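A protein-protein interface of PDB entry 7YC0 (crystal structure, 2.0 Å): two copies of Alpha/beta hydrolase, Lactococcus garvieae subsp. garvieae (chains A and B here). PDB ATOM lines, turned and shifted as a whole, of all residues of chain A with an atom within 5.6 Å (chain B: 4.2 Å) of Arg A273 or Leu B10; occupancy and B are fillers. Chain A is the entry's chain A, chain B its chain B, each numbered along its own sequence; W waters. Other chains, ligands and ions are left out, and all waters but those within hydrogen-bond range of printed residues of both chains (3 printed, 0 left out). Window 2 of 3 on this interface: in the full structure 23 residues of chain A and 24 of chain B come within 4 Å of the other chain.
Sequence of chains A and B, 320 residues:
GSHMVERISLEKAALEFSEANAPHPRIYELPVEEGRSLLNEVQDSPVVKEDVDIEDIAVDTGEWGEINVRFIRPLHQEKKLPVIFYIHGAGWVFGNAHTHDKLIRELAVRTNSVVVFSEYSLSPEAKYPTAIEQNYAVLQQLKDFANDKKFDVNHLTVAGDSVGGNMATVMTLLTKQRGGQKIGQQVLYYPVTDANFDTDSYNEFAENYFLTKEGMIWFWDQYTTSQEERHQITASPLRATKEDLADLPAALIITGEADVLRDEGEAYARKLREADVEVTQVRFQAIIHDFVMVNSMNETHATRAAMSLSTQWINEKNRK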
ATOM      1  N   TYR A 268      -6.985   3.394 -19.317  1.00  0.00           N
ATOM      2  CA  TYR A 268      -7.682   2.493 -20.269  1.00  0.00           C
ATOM      3  C   TYR A 268      -8.480   1.446 -19.481  1.00  0.00           C
ATOM      4  O   TYR A 268      -9.581   1.040 -19.909  1.00  0.00           O
ATOM      5  CB  TYR A 268      -6.692   1.826 -21.235  1.00  0.00           C
ATOM      6  CG  TYR A 268      -7.339   0.964 -22.301  1.00  0.00           C
ATOM      7  CD1 TYR A 268      -8.306   1.475 -23.155  1.00  0.00           C
ATOM      8  CD2 TYR A 268      -7.010  -0.374 -22.445  1.00  0.00           C
ATOM      9  CE1 TYR A 268      -8.908   0.694 -24.137  1.00  0.00           C
ATOM     10  CE2 TYR A 268      -7.593  -1.169 -23.426  1.00  0.00           C
ATOM     11  CZ  TYR A 268      -8.542  -0.633 -24.285  1.00  0.00           C
ATOM     12  OH  TYR A 268      -9.114  -1.396 -25.262  1.00  0.00           O
ATOM     13  N   ALA A 269      -7.899   0.960 -18.385  1.00  0.00           N
ATOM     14  CA  ALA A 269      -8.530  -0.026 -17.482  1.00  0.00           C
ATOM     15  C   ALA A 269      -9.821   0.563 -16.940  1.00  0.00           C
ATOM     16  O   ALA A 269     -10.820  -0.165 -16.907  1.00  0.00           O
ATOM     17  CB  ALA A 269      -7.614  -0.413 -16.346  1.00  0.00           C
ATOM     18  N   ARG A 270      -9.802   1.830 -16.542  1.00  0.00           N
ATOM     19  CA  ARG A 270     -11.016   2.473 -15.977  1.00  0.00           C
ATOM     20  C   ARG A 270     -12.069   2.592 -17.083  1.00  0.00           C
ATOM     21  O   ARG A 270     -13.228   2.310 -16.797  1.00  0.00           O
ATOM     22  CB  ARG A 270     -10.733   3.842 -15.369  1.00  0.00           C
ATOM     23  CG  ARG A 270      -9.958   3.799 -14.057  1.00  0.00           C
ATOM     24  CD  ARG A 270      -9.399   5.175 -13.712  1.00  0.00           C
ATOM     25  NE  ARG A 270      -9.054   5.341 -12.307  1.00  0.00           N
ATOM     26  CZ  ARG A 270      -8.516   6.433 -11.797  1.00  0.00           C
ATOM     27  NH1 ARG A 270      -8.232   7.452 -12.589  1.00  0.00           N
ATOM     28  NH2 ARG A 270      -8.274   6.512 -10.499  1.00  0.00           N
ATOM     29  N   LYS A 271     -11.682   2.977 -18.305  1.00  0.00           N
ATOM     30  CA  LYS A 271     -12.640   3.083 -19.449  1.00  0.00           C
ATOM     31  C   LYS A 271     -13.297   1.711 -19.727  1.00  0.00           C
ATOM     32  O   LYS A 271     -14.553   1.703 -19.819  1.00  0.00           O
ATOM     33  CB  LYS A 271     -11.987   3.690 -20.687  1.00  0.00           C
ATOM     34  CG  LYS A 271     -11.714   5.188 -20.591  1.00  0.00           C
ATOM     35  CD  LYS A 271     -11.522   5.826 -21.951  1.00  0.00           C
ATOM     36  CE  LYS A 271     -11.417   7.341 -21.952  1.00  0.00           C
ATOM     37  NZ  LYS A 271     -11.602   7.839 -23.331  1.00  0.00           N
ATOM     38  N   LEU A 272     -12.530   0.597 -19.800  1.00  0.00           N
ATOM     39  CA  LEU A 272     -13.118  -0.761 -19.979  1.00  0.00           C
ATOM     40  C   LEU A 272     -14.109  -1.021 -18.842  1.00  0.00           C
ATOM     41  O   LEU A 272     -15.209  -1.474 -19.146  1.00  0.00           O
ATOM     42  CB  LEU A 272     -12.046  -1.845 -20.026  1.00  0.00           C
ATOM     43  CG  LEU A 272     -11.076  -1.791 -21.200  1.00  0.00           C
ATOM     44  CD1 LEU A 272      -9.870  -2.681 -20.917  1.00  0.00           C
ATOM     45  CD2 LEU A 272     -11.744  -2.230 -22.499  1.00  0.00           C
ATOM     46  N   ARG A 273     -13.728  -0.768 -17.580  1.00  0.00           N
ATOM     47  CA  ARG A 273     -14.565  -1.046 -16.382  1.00  0.00           C
ATOM     48  C   ARG A 273     -15.866  -0.239 -16.482  1.00  0.00           C
ATOM     49  O   ARG A 273     -16.925  -0.818 -16.191  1.00  0.00           O
ATOM     50  CB  ARG A 273     -13.793  -0.754 -15.085  1.00  0.00           C
ATOM     51  CG  ARG A 273     -14.602  -0.890 -13.797  1.00  0.00           C
ATOM     52  CD  ARG A 273     -13.780  -0.745 -12.519  1.00  0.00           C
ATOM     53  NE  ARG A 273     -12.484  -1.410 -12.557  1.00  0.00           N
ATOM     54  CZ  ARG A 273     -11.311  -0.814 -12.743  1.00  0.00           C
ATOM     55  NH1 ARG A 273     -10.226  -1.547 -12.801  1.00  0.00           N
ATOM     56  NH2 ARG A 273     -11.211   0.498 -12.883  1.00  0.00           N
ATOM     57  N   GLU A 274     -15.788   1.042 -16.869  1.00  0.00           N
ATOM     58  CA  GLU A 274     -16.966   1.928 -17.069  1.00  0.00           C
ATOM     59  C   GLU A 274     -17.856   1.358 -18.186  1.00  0.00           C
ATOM     60  O   GLU A 274     -19.087   1.604 -18.126  1.00  0.00           O
ATOM     61  CB  GLU A 274     -16.518   3.384 -17.305  1.00  0.00           C
ATOM     62  CG  GLU A 274     -15.977   4.053 -16.027  1.00  0.00           C
ATOM     63  CD  GLU A 274     -14.977   5.218 -16.118  1.00  0.00           C
ATOM     64  OE1 GLU A 274     -14.519   5.554 -17.239  1.00  0.00           O
ATOM     65  OE2 GLU A 274     -14.616   5.791 -15.042  1.00  0.00           O
ATOM     66  N   ALA A 275     -17.308   0.600 -19.148  1.00  0.00           N
ATOM     67  CA  ALA A 275     -18.088  -0.012 -20.256  1.00  0.00           C
ATOM     68  C   ALA A 275     -18.582  -1.414 -19.881  1.00  0.00           C
ATOM     69  O   ALA A 275     -19.008  -2.154 -20.792  1.00  0.00           O
ATOM     70  CB  ALA A 275     -17.249  -0.085 -21.495  1.00  0.00           C
ATOM     71  N   ASP A 276     -18.448  -1.778 -18.602  1.00  0.00           N
ATOM     72  CA  ASP A 276     -18.948  -3.031 -17.973  1.00  0.00           C
ATOM     73  C   ASP A 276     -18.126  -4.227 -18.449  1.00  0.00           C
ATOM     74  O   ASP A 276     -18.578  -5.343 -18.215  1.00  0.00           O
ATOM     75  CB  ASP A 276     -20.448  -3.259 -18.201  1.00  0.00           C
ATOM     76  CG  ASP A 276     -21.309  -2.167 -17.603  1.00  0.00           C
ATOM     77  OD1 ASP A 276     -21.286  -2.020 -16.375  1.00  0.00           O
ATOM     78  OD2 ASP A 276     -21.953  -1.443 -18.383  1.00  0.00           O
ATOM     79  N   VAL A 277     -16.942  -4.010 -19.030  1.00  0.00           N
ATOM     80  CA  VAL A 277     -15.981  -5.106 -19.334  1.00  0.00           C
ATOM     81  C   VAL A 277     -15.374  -5.549 -17.998  1.00  0.00           C
ATOM     82  O   VAL A 277     -15.156  -4.693 -17.127  1.00  0.00           O
ATOM     83  CB  VAL A 277     -14.900  -4.665 -20.342  1.00  0.00           C
ATOM     84  CG1 VAL A 277     -13.787  -5.687 -20.515  1.00  0.00           C
ATOM     85  CG2 VAL A 277     -15.505  -4.304 -21.689  1.00  0.00           C
ATOM     86  N   VAL A 279     -12.548  -6.332 -15.676  1.00  0.00           N
ATOM     87  CA  VAL A 279     -11.168  -5.767 -15.655  1.00  0.00           C
ATOM     88  C   VAL A 279     -10.468  -6.142 -14.346  1.00  0.00           C
ATOM     89  O   VAL A 279     -10.990  -5.846 -13.234  1.00  0.00           O
ATOM     90  CB  VAL A 279     -11.172  -4.236 -15.875  1.00  0.00           C
ATOM     91  CG1 VAL A 279      -9.759  -3.677 -15.886  1.00  0.00           C
ATOM     92  CG2 VAL A 279     -11.873  -3.851 -17.164  1.00  0.00           C
ATOM     93  N   THR A 280      -9.287  -6.731 -14.477  1.00  0.00           N
ATOM     94  CA  THR A 280      -8.314  -6.931 -13.378  1.00  0.00           C
ATOM     95  C   THR A 280      -7.138  -6.017 -13.675  1.00  0.00           C
ATOM     96  O   THR A 280      -6.425  -6.284 -14.641  1.00  0.00           O
ATOM     97  CB  THR A 280      -7.872  -8.401 -13.272  1.00  0.00           C
ATOM     98  OG1 THR A 280      -9.034  -9.206 -13.090  1.00  0.00           O
ATOM     99  CG2 THR A 280      -6.909  -8.650 -12.134  1.00  0.00           C
ATOM    100  N   GLN A 281      -6.976  -4.954 -12.893  1.00  0.00           N
ATOM    101  CA  GLN A 281      -5.867  -3.979 -13.087  1.00  0.00           C
ATOM    102  C   GLN A 281      -4.968  -4.008 -11.845  1.00  0.00           C
ATOM    103  O   GLN A 281      -5.451  -3.842 -10.706  1.00  0.00           O
ATOM    104  CB  GLN A 281      -6.405  -2.587 -13.451  1.00  0.00           C
ATOM    105  CG  GLN A 281      -5.375  -1.704 -14.144  1.00  0.00           C
ATOM    106  CD  GLN A 281      -4.206  -1.344 -13.265  1.00  0.00           C
ATOM    107  OE1 GLN A 281      -4.394  -0.892 -12.136  1.00  0.00           O
ATOM    108  NE2 GLN A 281      -2.988  -1.548 -13.769  1.00  0.00           N
ATOM    109  N   ARG B   7     -17.222   9.483  -6.953  1.00  0.00           N
ATOM    110  CA  ARG B   7     -16.062   8.669  -6.525  1.00  0.00           C
ATOM    111  C   ARG B   7     -15.226   8.375  -7.764  1.00  0.00           C
ATOM    112  O   ARG B   7     -15.787   8.456  -8.868  1.00  0.00           O
ATOM    113  CB  ARG B   7     -16.545   7.363  -5.892  1.00  0.00           C
ATOM    114  CG  ARG B   7     -17.407   7.540  -4.652  1.00  0.00           C
ATOM    115  CD  ARG B   7     -17.841   6.206  -4.092  1.00  0.00           C
ATOM    116  NE  ARG B   7     -18.442   6.371  -2.787  1.00  0.00           N
ATOM    117  CZ  ARG B   7     -19.725   6.646  -2.557  1.00  0.00           C
ATOM    118  NH1 ARG B   7     -20.156   6.779  -1.310  1.00  0.00           N
ATOM    119  NH2 ARG B   7     -20.568   6.776  -3.560  1.00  0.00           N
ATOM    120  N   ILE B   8     -13.957   7.994  -7.591  1.00  0.00           N
ATOM    121  CA  ILE B   8     -13.165   7.420  -8.718  1.00  0.00           C
ATOM    122  C   ILE B   8     -13.832   6.102  -9.143  1.00  0.00           C
ATOM    123  O   ILE B   8     -14.668   5.572  -8.359  1.00  0.00           O
ATOM    124  CB  ILE B   8     -11.686   7.259  -8.343  1.00  0.00           C
ATOM    125  CG1 ILE B   8     -11.475   6.293  -7.181  1.00  0.00           C
ATOM    126  CG2 ILE B   8     -11.074   8.617  -8.047  1.00  0.00           C
ATOM    127  CD1 ILE B   8     -10.072   5.782  -7.085  1.00  0.00           C
ATOM    128  N   SER B   9     -13.536   5.628 -10.352  1.00  0.00           N
ATOM    129  CA  SER B   9     -13.924   4.272 -10.832  1.00  0.00           C
ATOM    130  C   SER B   9     -13.638   3.247  -9.727  1.00  0.00           C
ATOM    131  O   SER B   9     -12.458   3.155  -9.265  1.00  0.00           O
ATOM    132  CB  SER B   9     -13.229   3.880 -12.115  1.00  0.00           C
ATOM    133  OG  SER B   9     -13.390   2.479 -12.356  1.00  0.00           O
ATOM    134  N   LEU B  10     -14.682   2.534  -9.298  1.00  0.00           N
ATOM    135  CA  LEU B  10     -14.622   1.411  -8.312  1.00  0.00           C
ATOM    136  C   LEU B  10     -15.336   0.197  -8.907  1.00  0.00           C
ATOM    137  O   LEU B  10     -16.243   0.412  -9.676  1.00  0.00           O
ATOM    138  CB  LEU B  10     -15.328   1.817  -7.018  1.00  0.00           C
ATOM    139  CG  LEU B  10     -14.637   2.864  -6.141  1.00  0.00           C
ATOM    140  CD1 LEU B  10     -15.531   3.236  -4.955  1.00  0.00           C
ATOM    141  CD2 LEU B  10     -13.262   2.399  -5.667  1.00  0.00           C
ATOM    142  N   GLU B  11     -14.945  -1.016  -8.522  1.00  0.00           N
ATOM    143  CA  GLU B  11     -15.711  -2.274  -8.742  1.00  0.00           C
ATOM    144  C   GLU B  11     -17.079  -2.119  -8.071  1.00  0.00           C
ATOM    145  O   GLU B  11     -17.155  -1.444  -7.027  1.00  0.00           O
ATOM    146  CB  GLU B  11     -14.928  -3.470  -8.195  1.00  0.00           C
ATOM    147  CG  GLU B  11     -13.659  -3.726  -8.959  1.00  0.00           C
ATOM    148  CD  GLU B  11     -13.159  -5.157  -8.927  1.00  0.00           C
ATOM    149  OE1 GLU B  11     -12.005  -5.348  -8.522  1.00  0.00           O
ATOM    150  OE2 GLU B  11     -13.935  -6.078  -9.262  1.00  0.00           O
ATOM    151  N   LYS B  12     -18.119  -2.661  -8.698  1.00  0.00           N
ATOM    152  CA  LYS B  12     -19.534  -2.563  -8.256  1.00  0.00           C
ATOM    153  C   LYS B  12     -19.628  -2.864  -6.748  1.00  0.00           C
ATOM    154  O   LYS B  12     -20.140  -2.010  -6.005  1.00  0.00           O
ATOM    155  CB  LYS B  12     -20.376  -3.489  -9.134  1.00  0.00           C
ATOM    156  CG  LYS B  12     -21.856  -3.551  -8.780  1.00  0.00           C
ATOM    157  CD  LYS B  12     -22.783  -3.737  -9.974  1.00  0.00           C
ATOM    158  CE  LYS B  12     -22.737  -2.562 -10.937  1.00  0.00           C
ATOM    159  NZ  LYS B  12     -23.787  -2.654 -11.980  1.00  0.00           N
ATOM    160  N   LEU B  15     -18.193  -0.056  -4.617  1.00  0.00           N
ATOM    161  CA  LEU B  15     -19.093   1.126  -4.650  1.00  0.00           C
ATOM    162  C   LEU B  15     -20.252   0.870  -3.683  1.00  0.00           C
ATOM    163  O   LEU B  15     -20.618   1.787  -2.927  1.00  0.00           O
ATOM    164  CB  LEU B  15     -19.600   1.370  -6.078  1.00  0.00           C
ATOM    165  CG  LEU B  15     -20.631   2.494  -6.242  1.00  0.00           C
ATOM    166  CD1 LEU B  15     -20.144   3.808  -5.624  1.00  0.00           C
ATOM    167  CD2 LEU B  15     -20.962   2.688  -7.715  1.00  0.00           C
ATOM    168  N   TYR B 209     -15.323   6.224   0.939  1.00  0.00           N
ATOM    169  CA  TYR B 209     -14.703   4.943   0.522  1.00  0.00           C
ATOM    170  C   TYR B 209     -14.728   3.983   1.706  1.00  0.00           C
ATOM    171  O   TYR B 209     -13.766   3.228   1.895  1.00  0.00           O
ATOM    172  CB  TYR B 209     -13.309   5.207  -0.058  1.00  0.00           C
ATOM    173  CG  TYR B 209     -13.341   6.063  -1.296  1.00  0.00           C
ATOM    174  CD1 TYR B 209     -13.500   5.488  -2.550  1.00  0.00           C
ATOM    175  CD2 TYR B 209     -13.251   7.445  -1.220  1.00  0.00           C
ATOM    176  CE1 TYR B 209     -13.542   6.257  -3.696  1.00  0.00           C
ATOM    177  CE2 TYR B 209     -13.293   8.234  -2.365  1.00  0.00           C
ATOM    178  CZ  TYR B 209     -13.436   7.634  -3.604  1.00  0.00           C
ATOM    179  OH  TYR B 209     -13.490   8.375  -4.744  1.00  0.00           O
ATOM    180  N   ALA B 258      -8.209   2.842  -3.593  1.00  0.00           N
ATOM    181  CA  ALA B 258      -9.229   3.737  -2.989  1.00  0.00           C
ATOM    182  C   ALA B 258      -9.269   3.557  -1.466  1.00  0.00           C
ATOM    183  O   ALA B 258     -10.359   3.161  -0.923  1.00  0.00           O
ATOM    184  CB  ALA B 258     -10.577   3.446  -3.611  1.00  0.00           C
ATOM    185  N   GLN B 285      -6.297  -1.843  -8.482  1.00  0.00           N
ATOM    186  CA  GLN B 285      -7.064  -0.650  -8.917  1.00  0.00           C
ATOM    187  C   GLN B 285      -8.494  -0.752  -8.388  1.00  0.00           C
ATOM    188  O   GLN B 285      -8.999  -1.874  -8.277  1.00  0.00           O
ATOM    189  CB  GLN B 285      -7.071  -0.518 -10.450  1.00  0.00           C
ATOM    190  CG  GLN B 285      -7.286   0.922 -10.915  1.00  0.00           C
ATOM    191  CD  GLN B 285      -7.411   1.081 -12.415  1.00  0.00           C
ATOM    192  OE1 GLN B 285      -8.081   0.318 -13.114  1.00  0.00           O
ATOM    193  NE2 GLN B 285      -6.769   2.113 -12.927  1.00  0.00           N
ATOM    194  N   ALA B 286      -9.146   0.380  -8.138  1.00  0.00           N
ATOM    195  CA  ALA B 286     -10.629   0.467  -8.124  1.00  0.00           C
ATOM    196  C   ALA B 286     -11.215  -0.390  -7.005  1.00  0.00           C
ATOM    197  O   ALA B 286     -12.339  -0.942  -7.165  1.00  0.00           O
ATOM    198  CB  ALA B 286     -11.166   0.047  -9.479  1.00  0.00           C
ATOM    199  N   ILE B 287     -10.518  -0.456  -5.878  1.00  0.00           N
ATOM    200  CA  ILE B 287     -10.941  -1.265  -4.713  1.00  0.00           C
ATOM    201  C   ILE B 287     -10.674  -0.460  -3.446  1.00  0.00           C
ATOM    202  O   ILE B 287      -9.726   0.355  -3.403  1.00  0.00           O
ATOM    203  CB  ILE B 287     -10.258  -2.647  -4.691  1.00  0.00           C
ATOM    204  CG1 ILE B 287     -11.117  -3.697  -3.977  1.00  0.00           C
ATOM    205  CG2 ILE B 287      -8.876  -2.547  -4.082  1.00  0.00           C
ATOM    206  CD1 ILE B 287     -12.375  -4.095  -4.725  1.00  0.00           C
ATOM    207  N   ILE B 288     -11.533  -0.696  -2.473  1.00  0.00           N
ATOM    208  CA  ILE B 288     -11.559  -0.023  -1.147  1.00  0.00           C
ATOM    209  C   ILE B 288     -10.903  -0.925  -0.107  1.00  0.00           C
ATOM    210  O   ILE B 288     -10.596  -2.115  -0.399  1.00  0.00           O
ATOM    211  CB  ILE B 288     -13.008   0.309  -0.755  1.00  0.00           C
ATOM    212  CG1 ILE B 288     -13.870  -0.958  -0.661  1.00  0.00           C
ATOM    213  CG2 ILE B 288     -13.614   1.344  -1.703  1.00  0.00           C
ATOM    214  CD1 ILE B 288     -15.156  -0.746   0.111  1.00  0.00           C
HETATM  215  O   HOH W   1     -11.927   7.155 -12.092  1.00  0.00           O
HETATM  216  O   HOH W   2      -9.944   3.443 -10.401  1.00  0.00           O
HETATM  217  O   HOH W   3      -3.568  -0.065  -9.567  1.00  0.00           O
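The guanidinium group (NH2) of Arg A273 is in hydrogen-bond range of the side-chain hydroxyl (OG) of Ser B9 (3.0 Å).
NH1 of Arg A273 is in hydrogen-bond range of OE1 of Gln B285, 2.9 Å away.
The backbone carbonyl oxygen of Gln A281 is in hydrogen-bond range of the backbone NH of Gln B285, 3.1 Å away.
The side-chain hydroxyl (OH) of Tyr B209 sits at hydrogen-bond distance from the backbone NH (N) of Ile B8 (2.9 Å).
N of Glu B11 is in hydrogen-bond range of O of Ala B286.
Gln B285 touches Ala A269 (OE1 to CB, 3.3 Å).
Ile B8 touches Arg A270.
CG of Arg A270 touches CB of Ser B9 (3.8 Å).
Arg A270 touches Gln B285.
Arg A273 touches Leu B10.
Ala B286 touches Arg A273.
Glu A274 touches Ser B9.
Of the printed residues of chain B, Ala A269 touches Gln B285 (3.3 Å).
Of the printed residues of chain B, Arg A270 touches Ile B8 (3.9 Å), Ser B9 (3.8 Å) and Gln B285 (3.8 Å).
Arg A273 touches just these residues of chain B: Ser B9, Leu B10, Gln B285 and Ala B286.
Printed residues of chain B within 4 Å of Gln A281: Gln B285 (3.1 Å).
Leu B10 touches one residue of chain A.
Ala B258 touches none of the printed residues of chain A.
The nearest printed residue of chain B that does not touch Arg A273 is Glu B11 (4.2 Å).
The nearest printed residue of chain A that does not touch Leu B10 is Glu A274 (6.6 Å).
The nearest printed residue of chain B that does not touch Ala A269 is Ser B9 (5.9 Å).
Of the 13 printed residues of chain B, 5 touch a printed residue of chain A.
Of the 13 printed residues of chain A, 5 touch a printed residue of chain B.
Hydrophobic or aromatic side chains of chain A that line the printed part of chain B: Ala A269.
Among the printed residues, 10 pairs touch across the chains.
No position is printed for both chains.
Water W2 lies within hydrogen-bond range of the backbone carbonyl oxygen (O) of Ser B9 (2.8 Å) and the guanidinium group (NE) of Arg A270 (2.8 Å).
Water W1 bridges the backbone NH (N) of Ser B9 and the guanidinium group (NE) of Arg A270.
Water W3 bridges the side-chain amide oxygen of Gln A281 (2.8 Å) and the backbone NH of Gln B285 (3.4 Å).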
